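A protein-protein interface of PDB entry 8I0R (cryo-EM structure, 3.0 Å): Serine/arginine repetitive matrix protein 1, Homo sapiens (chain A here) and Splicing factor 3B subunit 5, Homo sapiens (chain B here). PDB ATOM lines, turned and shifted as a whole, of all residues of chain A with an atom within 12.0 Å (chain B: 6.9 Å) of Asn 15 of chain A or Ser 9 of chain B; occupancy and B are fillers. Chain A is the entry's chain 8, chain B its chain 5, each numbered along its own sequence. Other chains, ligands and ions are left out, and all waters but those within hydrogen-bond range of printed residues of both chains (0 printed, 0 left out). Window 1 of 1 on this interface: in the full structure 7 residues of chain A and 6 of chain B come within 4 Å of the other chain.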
ATOM      1  N   GLU A  12      22.992  -6.071 -16.746  1.00  0.00           N
ATOM      2  CA  GLU A  12      21.624  -5.569 -16.713  1.00  0.00           C
ATOM      3  C   GLU A  12      20.742  -6.364 -17.649  1.00  0.00           C
ATOM      4  O   GLU A  12      19.664  -6.811 -17.274  1.00  0.00           O
ATOM      5  CB  GLU A  12      21.579  -4.088 -17.091  1.00  0.00           C
ATOM      6  CG  GLU A  12      22.520  -3.694 -18.223  1.00  0.00           C
ATOM      7  CD  GLU A  12      22.054  -2.461 -18.965  1.00  0.00           C
ATOM      8  OE1 GLU A  12      22.352  -2.343 -20.169  1.00  0.00           O
ATOM      9  OE2 GLU A  12      21.389  -1.613 -18.341  1.00  0.00           O
ATOM     10  N   GLN A  13      21.203  -6.523 -18.884  1.00  0.00           N
ATOM     11  CA  GLN A  13      20.460  -7.263 -19.894  1.00  0.00           C
ATOM     12  C   GLN A  13      21.288  -8.383 -20.512  1.00  0.00           C
ATOM     13  O   GLN A  13      20.724  -9.343 -21.047  1.00  0.00           O
ATOM     14  CB  GLN A  13      19.966  -6.293 -20.968  1.00  0.00           C
ATOM     15  CG  GLN A  13      19.150  -5.147 -20.393  1.00  0.00           C
ATOM     16  CD  GLN A  13      19.261  -3.873 -21.203  1.00  0.00           C
ATOM     17  OE1 GLN A  13      20.285  -3.614 -21.833  1.00  0.00           O
ATOM     18  NE2 GLN A  13      18.211  -3.064 -21.182  1.00  0.00           N
ATOM     19  N   ASP A  14      22.615  -8.296 -20.427  1.00  0.00           N
ATOM     20  CA  ASP A  14      23.518  -9.233 -21.079  1.00  0.00           C
ATOM     21  C   ASP A  14      23.935 -10.335 -20.114  1.00  0.00           C
ATOM     22  O   ASP A  14      24.065 -10.107 -18.906  1.00  0.00           O
ATOM     23  CB  ASP A  14      24.762  -8.513 -21.613  1.00  0.00           C
ATOM     24  CG  ASP A  14      25.726  -9.443 -22.359  1.00  0.00           C
ATOM     25  OD1 ASP A  14      25.492 -10.670 -22.421  1.00  0.00           O
ATOM     26  OD2 ASP A  14      26.728  -8.934 -22.902  1.00  0.00           O
ATOM     27  N   ASN A  15      24.156 -11.527 -20.667  1.00  0.00           N
ATOM     28  CA  ASN A  15      24.583 -12.702 -19.920  1.00  0.00           C
ATOM     29  C   ASN A  15      26.002 -13.112 -20.290  1.00  0.00           C
ATOM     30  O   ASN A  15      26.683 -13.788 -19.519  1.00  0.00           O
ATOM     31  CB  ASN A  15      23.623 -13.863 -20.171  1.00  0.00           C
ATOM     32  CG  ASN A  15      23.545 -14.244 -21.635  1.00  0.00           C
ATOM     33  OD1 ASN A  15      24.232 -13.667 -22.475  1.00  0.00           O
ATOM     34  ND2 ASN A  15      22.707 -15.222 -21.947  1.00  0.00           N
ATOM     35  N   ARG A  16      26.453 -12.696 -21.472  1.00  0.00           N
ATOM     36  CA  ARG A  16      27.701 -13.168 -22.051  1.00  0.00           C
ATOM     37  C   ARG A  16      28.928 -12.422 -21.547  1.00  0.00           C
ATOM     38  O   ARG A  16      30.019 -12.627 -22.088  1.00  0.00           O
ATOM     39  CB  ARG A  16      27.638 -13.060 -23.579  1.00  0.00           C
ATOM     40  CG  ARG A  16      27.240 -14.353 -24.282  1.00  0.00           C
ATOM     41  CD  ARG A  16      27.266 -14.193 -25.798  1.00  0.00           C
ATOM     42  NE  ARG A  16      27.316 -12.786 -26.198  1.00  0.00           N
ATOM     43  CZ  ARG A  16      26.287 -12.096 -26.688  1.00  0.00           C
ATOM     44  NH1 ARG A  16      25.098 -12.667 -26.839  1.00  0.00           N
ATOM     45  NH2 ARG A  16      26.446 -10.821 -27.015  1.00  0.00           N
ATOM     46  N   PHE A  17      28.778 -11.559 -20.547  1.00  0.00           N
ATOM     47  CA  PHE A  17      29.902 -10.902 -19.896  1.00  0.00           C
ATOM     48  C   PHE A  17      29.847 -11.142 -18.394  1.00  0.00           C
ATOM     49  O   PHE A  17      28.764 -11.271 -17.815  1.00  0.00           O
ATOM     50  CB  PHE A  17      29.913  -9.403 -20.194  1.00  0.00           C
ATOM     51  CG  PHE A  17      30.732  -9.028 -21.398  1.00  0.00           C
ATOM     52  CD1 PHE A  17      31.805  -9.804 -21.785  1.00  0.00           C
ATOM     53  CD2 PHE A  17      30.429  -7.899 -22.136  1.00  0.00           C
ATOM     54  CE1 PHE A  17      32.552  -9.460 -22.881  1.00  0.00           C
ATOM     55  CE2 PHE A  17      31.172  -7.558 -23.231  1.00  0.00           C
ATOM     56  CZ  PHE A  17      32.237  -8.334 -23.603  1.00  0.00           C
ATOM     57  N   SER A  18      31.019 -11.207 -17.771  1.00  0.00           N
ATOM     58  CA  SER A  18      31.142 -11.519 -16.354  1.00  0.00           C
ATOM     59  C   SER A  18      31.317 -10.254 -15.520  1.00  0.00           C
ATOM     60  O   SER A  18      31.688  -9.198 -16.039  1.00  0.00           O
ATOM     61  CB  SER A  18      32.320 -12.460 -16.130  1.00  0.00           C
ATOM     62  OG  SER A  18      33.417 -12.100 -16.951  1.00  0.00           O
ATOM     63  N   ASN A  19      31.038 -10.361 -14.223  1.00  0.00           N
ATOM     64  CA  ASN A  19      31.226  -9.222 -13.329  1.00  0.00           C
ATOM     65  C   ASN A  19      32.706  -9.072 -13.010  1.00  0.00           C
ATOM     66  O   ASN A  19      33.261  -9.818 -12.187  1.00  0.00           O
ATOM     67  CB  ASN A  19      30.415  -9.384 -12.051  1.00  0.00           C
ATOM     68  CG  ASN A  19      30.669  -8.257 -11.066  1.00  0.00           C
ATOM     69  OD1 ASN A  19      30.690  -8.465  -9.857  1.00  0.00           O
ATOM     70  ND2 ASN A  19      30.877  -7.053 -11.589  1.00  0.00           N
ATOM     71  N   LYS A  20      33.343  -8.080 -13.631  1.00  0.00           N
ATOM     72  CA  LYS A  20      34.778  -7.928 -13.466  1.00  0.00           C
ATOM     73  C   LYS A  20      35.142  -7.493 -12.062  1.00  0.00           C
ATOM     74  O   LYS A  20      36.210  -7.878 -11.566  1.00  0.00           O
ATOM     75  CB  LYS A  20      35.319  -6.943 -14.496  1.00  0.00           C
ATOM     76  CG  LYS A  20      35.008  -7.343 -15.938  1.00  0.00           C
ATOM     77  CD  LYS A  20      35.182  -8.841 -16.169  1.00  0.00           C
ATOM     78  CE  LYS A  20      34.820  -9.238 -17.591  1.00  0.00           C
ATOM     79  NZ  LYS A  20      33.575  -8.582 -18.067  1.00  0.00           N
ATOM     80  N   GLN A  21      34.275  -6.726 -11.398  1.00  0.00           N
ATOM     81  CA  GLN A  21      34.523  -6.407  -9.997  1.00  0.00           C
ATOM     82  C   GLN A  21      34.658  -7.675  -9.169  1.00  0.00           C
ATOM     83  O   GLN A  21      35.690  -7.893  -8.538  1.00  0.00           O
ATOM     84  CB  GLN A  21      33.438  -5.490  -9.440  1.00  0.00           C
ATOM     85  CG  GLN A  21      33.486  -4.092 -10.029  1.00  0.00           C
ATOM     86  CD  GLN A  21      32.148  -3.600 -10.528  1.00  0.00           C
ATOM     87  OE1 GLN A  21      31.112  -4.222 -10.286  1.00  0.00           O
ATOM     88  NE2 GLN A  21      32.158  -2.463 -11.218  1.00  0.00           N
ATOM     89  N   LYS A  22      33.628  -8.525  -9.162  1.00  0.00           N
ATOM     90  CA  LYS A  22      33.719  -9.790  -8.432  1.00  0.00           C
ATOM     91  C   LYS A  22      34.962 -10.577  -8.820  1.00  0.00           C
ATOM     92  O   LYS A  22      35.584 -11.233  -7.971  1.00  0.00           O
ATOM     93  CB  LYS A  22      32.477 -10.640  -8.671  1.00  0.00           C
ATOM     94  CG  LYS A  22      31.447 -10.580  -7.563  1.00  0.00           C
ATOM     95  CD  LYS A  22      30.092 -11.090  -8.027  1.00  0.00           C
ATOM     96  CE  LYS A  22      30.187 -12.271  -8.991  1.00  0.00           C
ATOM     97  NZ  LYS A  22      31.062 -13.387  -8.527  1.00  0.00           N
ATOM     98  N   LYS A  23      35.337 -10.543 -10.100  1.00  0.00           N
ATOM     99  CA  LYS A  23      36.524 -11.291 -10.503  1.00  0.00           C
ATOM    100  C   LYS A  23      37.776 -10.744  -9.819  1.00  0.00           C
ATOM    101  O   LYS A  23      38.631 -11.508  -9.358  1.00  0.00           O
ATOM    102  CB  LYS A  23      36.654 -11.288 -12.025  1.00  0.00           C
ATOM    103  CG  LYS A  23      35.560 -12.101 -12.715  1.00  0.00           C
ATOM    104  CD  LYS A  23      35.032 -13.196 -11.785  1.00  0.00           C
ATOM    105  CE  LYS A  23      34.142 -14.208 -12.488  1.00  0.00           C
ATOM    106  NZ  LYS A  23      32.940 -13.599 -13.096  1.00  0.00           N
ATOM    107  N   ASP B   3      35.069 -20.452 -24.476  1.00  0.00           N
ATOM    108  CA  ASP B   3      33.784 -21.080 -24.190  1.00  0.00           C
ATOM    109  C   ASP B   3      33.607 -21.287 -22.699  1.00  0.00           C
ATOM    110  O   ASP B   3      32.518 -21.063 -22.156  1.00  0.00           O
ATOM    111  CB  ASP B   3      33.649 -22.408 -24.934  1.00  0.00           C
ATOM    112  CG  ASP B   3      33.881 -22.269 -26.415  1.00  0.00           C
ATOM    113  OD1 ASP B   3      33.742 -21.142 -26.931  1.00  0.00           O
ATOM    114  OD2 ASP B   3      34.191 -23.290 -27.064  1.00  0.00           O
ATOM    115  N   ARG B   4      34.688 -21.659 -22.010  1.00  0.00           N
ATOM    116  CA  ARG B   4      34.614 -21.909 -20.575  1.00  0.00           C
ATOM    117  C   ARG B   4      34.016 -20.716 -19.842  1.00  0.00           C
ATOM    118  O   ARG B   4      32.918 -20.805 -19.277  1.00  0.00           O
ATOM    119  CB  ARG B   4      36.011 -22.233 -20.039  1.00  0.00           C
ATOM    120  CG  ARG B   4      36.073 -22.608 -18.571  1.00  0.00           C
ATOM    121  CD  ARG B   4      36.330 -21.391 -17.695  1.00  0.00           C
ATOM    122  NE  ARG B   4      36.328 -21.724 -16.276  1.00  0.00           N
ATOM    123  CZ  ARG B   4      35.228 -21.881 -15.545  1.00  0.00           C
ATOM    124  NH1 ARG B   4      34.033 -21.742 -16.102  1.00  0.00           N
ATOM    125  NH2 ARG B   4      35.325 -22.185 -14.258  1.00  0.00           N
ATOM    126  N   TYR B   5      34.702 -19.577 -19.870  1.00  0.00           N
ATOM    127  CA  TYR B   5      34.182 -18.470 -19.085  1.00  0.00           C
ATOM    128  C   TYR B   5      33.017 -17.752 -19.755  1.00  0.00           C
ATOM    129  O   TYR B   5      32.309 -17.012 -19.072  1.00  0.00           O
ATOM    130  CB  TYR B   5      35.285 -17.476 -18.724  1.00  0.00           C
ATOM    131  CG  TYR B   5      35.557 -17.436 -17.230  1.00  0.00           C
ATOM    132  CD1 TYR B   5      36.667 -18.068 -16.685  1.00  0.00           C
ATOM    133  CD2 TYR B   5      34.689 -16.783 -16.363  1.00  0.00           C
ATOM    134  CE1 TYR B   5      36.913 -18.032 -15.323  1.00  0.00           C
ATOM    135  CE2 TYR B   5      34.928 -16.745 -14.998  1.00  0.00           C
ATOM    136  CZ  TYR B   5      36.042 -17.371 -14.486  1.00  0.00           C
ATOM    137  OH  TYR B   5      36.280 -17.333 -13.131  1.00  0.00           O
ATOM    138  N   THR B   6      32.734 -17.976 -21.044  1.00  0.00           N
ATOM    139  CA  THR B   6      31.534 -17.329 -21.574  1.00  0.00           C
ATOM    140  C   THR B   6      30.271 -18.074 -21.151  1.00  0.00           C
ATOM    141  O   THR B   6      29.233 -17.450 -20.872  1.00  0.00           O
ATOM    142  CB  THR B   6      31.590 -17.182 -23.093  1.00  0.00           C
ATOM    143  OG1 THR B   6      30.449 -16.432 -23.523  1.00  0.00           O
ATOM    144  CG2 THR B   6      31.536 -18.516 -23.777  1.00  0.00           C
ATOM    145  N   ILE B   7      30.334 -19.405 -21.044  1.00  0.00           N
ATOM    146  CA  ILE B   7      29.154 -20.054 -20.492  1.00  0.00           C
ATOM    147  C   ILE B   7      29.159 -19.932 -18.980  1.00  0.00           C
ATOM    148  O   ILE B   7      28.094 -19.947 -18.359  1.00  0.00           O
ATOM    149  CB  ILE B   7      29.000 -21.516 -20.958  1.00  0.00           C
ATOM    150  CG1 ILE B   7      30.272 -22.335 -20.744  1.00  0.00           C
ATOM    151  CG2 ILE B   7      28.533 -21.554 -22.415  1.00  0.00           C
ATOM    152  CD1 ILE B   7      30.187 -23.727 -21.328  1.00  0.00           C
ATOM    153  N   HIS B   8      30.336 -19.777 -18.360  1.00  0.00           N
ATOM    154  CA  HIS B   8      30.368 -19.390 -16.950  1.00  0.00           C
ATOM    155  C   HIS B   8      29.673 -18.049 -16.746  1.00  0.00           C
ATOM    156  O   HIS B   8      28.966 -17.853 -15.751  1.00  0.00           O
ATOM    157  CB  HIS B   8      31.812 -19.340 -16.450  1.00  0.00           C
ATOM    158  CG  HIS B   8      31.944 -19.364 -14.959  1.00  0.00           C
ATOM    159  ND1 HIS B   8      33.122 -19.694 -14.324  1.00  0.00           N
ATOM    160  CD2 HIS B   8      31.045 -19.112 -13.977  1.00  0.00           C
ATOM    161  CE1 HIS B   8      32.947 -19.636 -13.017  1.00  0.00           C
ATOM    162  NE2 HIS B   8      31.696 -19.287 -12.779  1.00  0.00           N
ATOM    163  N   SER B   9      29.817 -17.144 -17.716  1.00  0.00           N
ATOM    164  CA  SER B   9      29.084 -15.885 -17.717  1.00  0.00           C
ATOM    165  C   SER B   9      27.583 -16.116 -17.771  1.00  0.00           C
ATOM    166  O   SER B   9      26.835 -15.631 -16.906  1.00  0.00           O
ATOM    167  CB  SER B   9      29.526 -15.049 -18.917  1.00  0.00           C
ATOM    168  OG  SER B   9      28.833 -13.819 -18.963  1.00  0.00           O
ATOM    169  N   GLN B  10      27.123 -16.819 -18.809  1.00  0.00           N
ATOM    170  CA  GLN B  10      25.688 -17.028 -18.977  1.00  0.00           C
ATOM    171  C   GLN B  10      25.078 -17.745 -17.775  1.00  0.00           C
ATOM    172  O   GLN B  10      23.933 -17.462 -17.401  1.00  0.00           O
ATOM    173  CB  GLN B  10      25.413 -17.807 -20.259  1.00  0.00           C
ATOM    174  CG  GLN B  10      25.992 -17.185 -21.507  1.00  0.00           C
ATOM    175  CD  GLN B  10      25.564 -17.918 -22.761  1.00  0.00           C
ATOM    176  OE1 GLN B  10      25.154 -19.075 -22.698  1.00  0.00           O
ATOM    177  NE2 GLN B  10      25.657 -17.253 -23.906  1.00  0.00           N
ATOM    178  N   LEU B  11      25.826 -18.651 -17.134  1.00  0.00           N
ATOM    179  CA  LEU B  11      25.271 -19.377 -15.996  1.00  0.00           C
ATOM    180  C   LEU B  11      25.285 -18.536 -14.730  1.00  0.00           C
ATOM    181  O   LEU B  11      24.379 -18.659 -13.902  1.00  0.00           O
ATOM    182  CB  LEU B  11      26.018 -20.688 -15.754  1.00  0.00           C
ATOM    183  CG  LEU B  11      27.522 -20.677 -15.470  1.00  0.00           C
ATOM    184  CD1 LEU B  11      27.869 -20.407 -14.013  1.00  0.00           C
ATOM    185  CD2 LEU B  11      28.154 -21.975 -15.958  1.00  0.00           C
ATOM    186  N   GLU B  12      26.311 -17.699 -14.539  1.00  0.00           N
ATOM    187  CA  GLU B  12      26.258 -16.736 -13.447  1.00  0.00           C
ATOM    188  C   GLU B  12      25.016 -15.872 -13.572  1.00  0.00           C
ATOM    189  O   GLU B  12      24.306 -15.642 -12.586  1.00  0.00           O
ATOM    190  CB  GLU B  12      27.527 -15.880 -13.441  1.00  0.00           C
ATOM    191  CG  GLU B  12      27.931 -15.335 -12.076  1.00  0.00           C
ATOM    192  CD  GLU B  12      27.140 -14.109 -11.673  1.00  0.00           C
ATOM    193  OE1 GLU B  12      26.402 -13.571 -12.518  1.00  0.00           O
ATOM    194  OE2 GLU B  12      27.273 -13.667 -10.517  1.00  0.00           O
ATOM    195  N   HIS B  13      24.725 -15.421 -14.795  1.00  0.00           N
ATOM    196  CA  HIS B  13      23.516 -14.651 -15.074  1.00  0.00           C
ATOM    197  C   HIS B  13      22.254 -15.430 -14.723  1.00  0.00           C
ATOM    198  O   HIS B  13      21.410 -14.949 -13.952  1.00  0.00           O
ATOM    199  CB  HIS B  13      23.497 -14.267 -16.552  1.00  0.00           C
ATOM    200  CG  HIS B  13      22.956 -12.901 -16.816  1.00  0.00           C
ATOM    201  ND1 HIS B  13      21.835 -12.680 -17.586  1.00  0.00           N
ATOM    202  CD2 HIS B  13      23.383 -11.683 -16.411  1.00  0.00           C
ATOM    203  CE1 HIS B  13      21.593 -11.383 -17.641  1.00  0.00           C
ATOM    204  NE2 HIS B  13      22.519 -10.755 -16.939  1.00  0.00           N
ATOM    205  N   LEU B  14      22.103 -16.621 -15.307  1.00  0.00           N
ATOM    206  CA  LEU B  14      20.953 -17.460 -15.003  1.00  0.00           C
ATOM    207  C   LEU B  14      20.762 -17.597 -13.514  1.00  0.00           C
ATOM    208  O   LEU B  14      19.691 -17.283 -13.004  1.00  0.00           O
ATOM    209  CB  LEU B  14      21.099 -18.841 -15.631  1.00  0.00           C
ATOM    210  CG  LEU B  14      20.208 -19.005 -16.853  1.00  0.00           C
ATOM    211  CD1 LEU B  14      19.936 -20.459 -17.107  1.00  0.00           C
ATOM    212  CD2 LEU B  14      18.916 -18.230 -16.680  1.00  0.00           C
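Of the 12 printed residues of chain A, 7 touch a printed residue of chain B. Among the printed residues, 11 pairs touch across the chains. Among the printed residues, no Asp or Glu carboxylate lies within 4 Å of a Lys or Arg side-chain nitrogen of the other chain.
OG of Ser 9 of chain B sits at hydrogen-bond distance from N of Phe 17 of chain A. O of Asn 15 of chain A sits at hydrogen-bond distance from N of Gln 10 of chain B. NE2 of His 13 of chain B is in hydrogen-bond range of O of Asp 14 of chain A, at 2.6 Å. The backbone carbonyl oxygen of Asn 15 of chain A lies close to the side-chain hydroxyl of Ser 9 of chain B, at 2.2 Å.
Of the printed residues of chain B, Phe 17 of chain A touches Ser 9 (2.8 Å). Of the printed residues of chain B, Ser 18 of chain A touches Ser 9. Asn 19 of chain A touches none of the printed residues of chain B. Of the printed residues of chain B, Lys 23 of chain A touches Tyr 5. Printed residues of chain A within 4 Å of Tyr 5 of chain B: Lys 23 (3.7 Å). Of the printed residues of chain A, Thr 6 of chain B touches Arg 16. No residue of chain A comes within 4 Å of Ile 7 of chain B. No residue of chain A comes within 4 Å of His 8 of chain B. Ser 9 of chain B touches just these residues of chain A: Asn 15, Arg 16, Phe 17 and Ser 18. Of chain A, only Lys 22 comes within 4 Å of Glu 12 of chain B. Of the printed residues of chain A, His 13 of chain B touches Asp 14 (2.6 Å) and Asn 15 (3.4 Å). The nearest residue of chain B that does not touch Asn 15 of chain A is Thr 6 of chain B (4.7 Å).
The side-chain carboxylate of Asp 14 of chain A lies close to the side-chain amide oxygen of Asn 15 of chain A (3.3 Å). N of Arg 16 of chain A is in hydrogen-bond range of OD1 of Asp 14 of chain A (2.4 Å). The side-chain amino group (NZ) of Lys 20 of chain A is in hydrogen-bond range of the backbone carbonyl oxygen (O) of Ser 18 of chain A (2.8 Å). OD1 of Asn 19 of chain A is in hydrogen-bond range of N of Lys 22 of chain A (3.0 Å).
Among the printed residues, pairs that only touch across the chains: Arg 16 of chain A with Ser 9 of chain B (2.9 Å), Arg 16 of chain A with Gln 10 of chain B (3.3 Å), Asn 15 of chain A with His 13 of chain B (3.4 Å), Lys 22 of chain A with Glu 12 of chain B (3.6 Å), Ser 18 of chain A with Ser 9 of chain B (3.6 Å), Lys 23 of chain A with Tyr 5 of chain B (3.7 Å) and Arg 16 of chain A with Thr 6 of chain B (3.9 Å).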
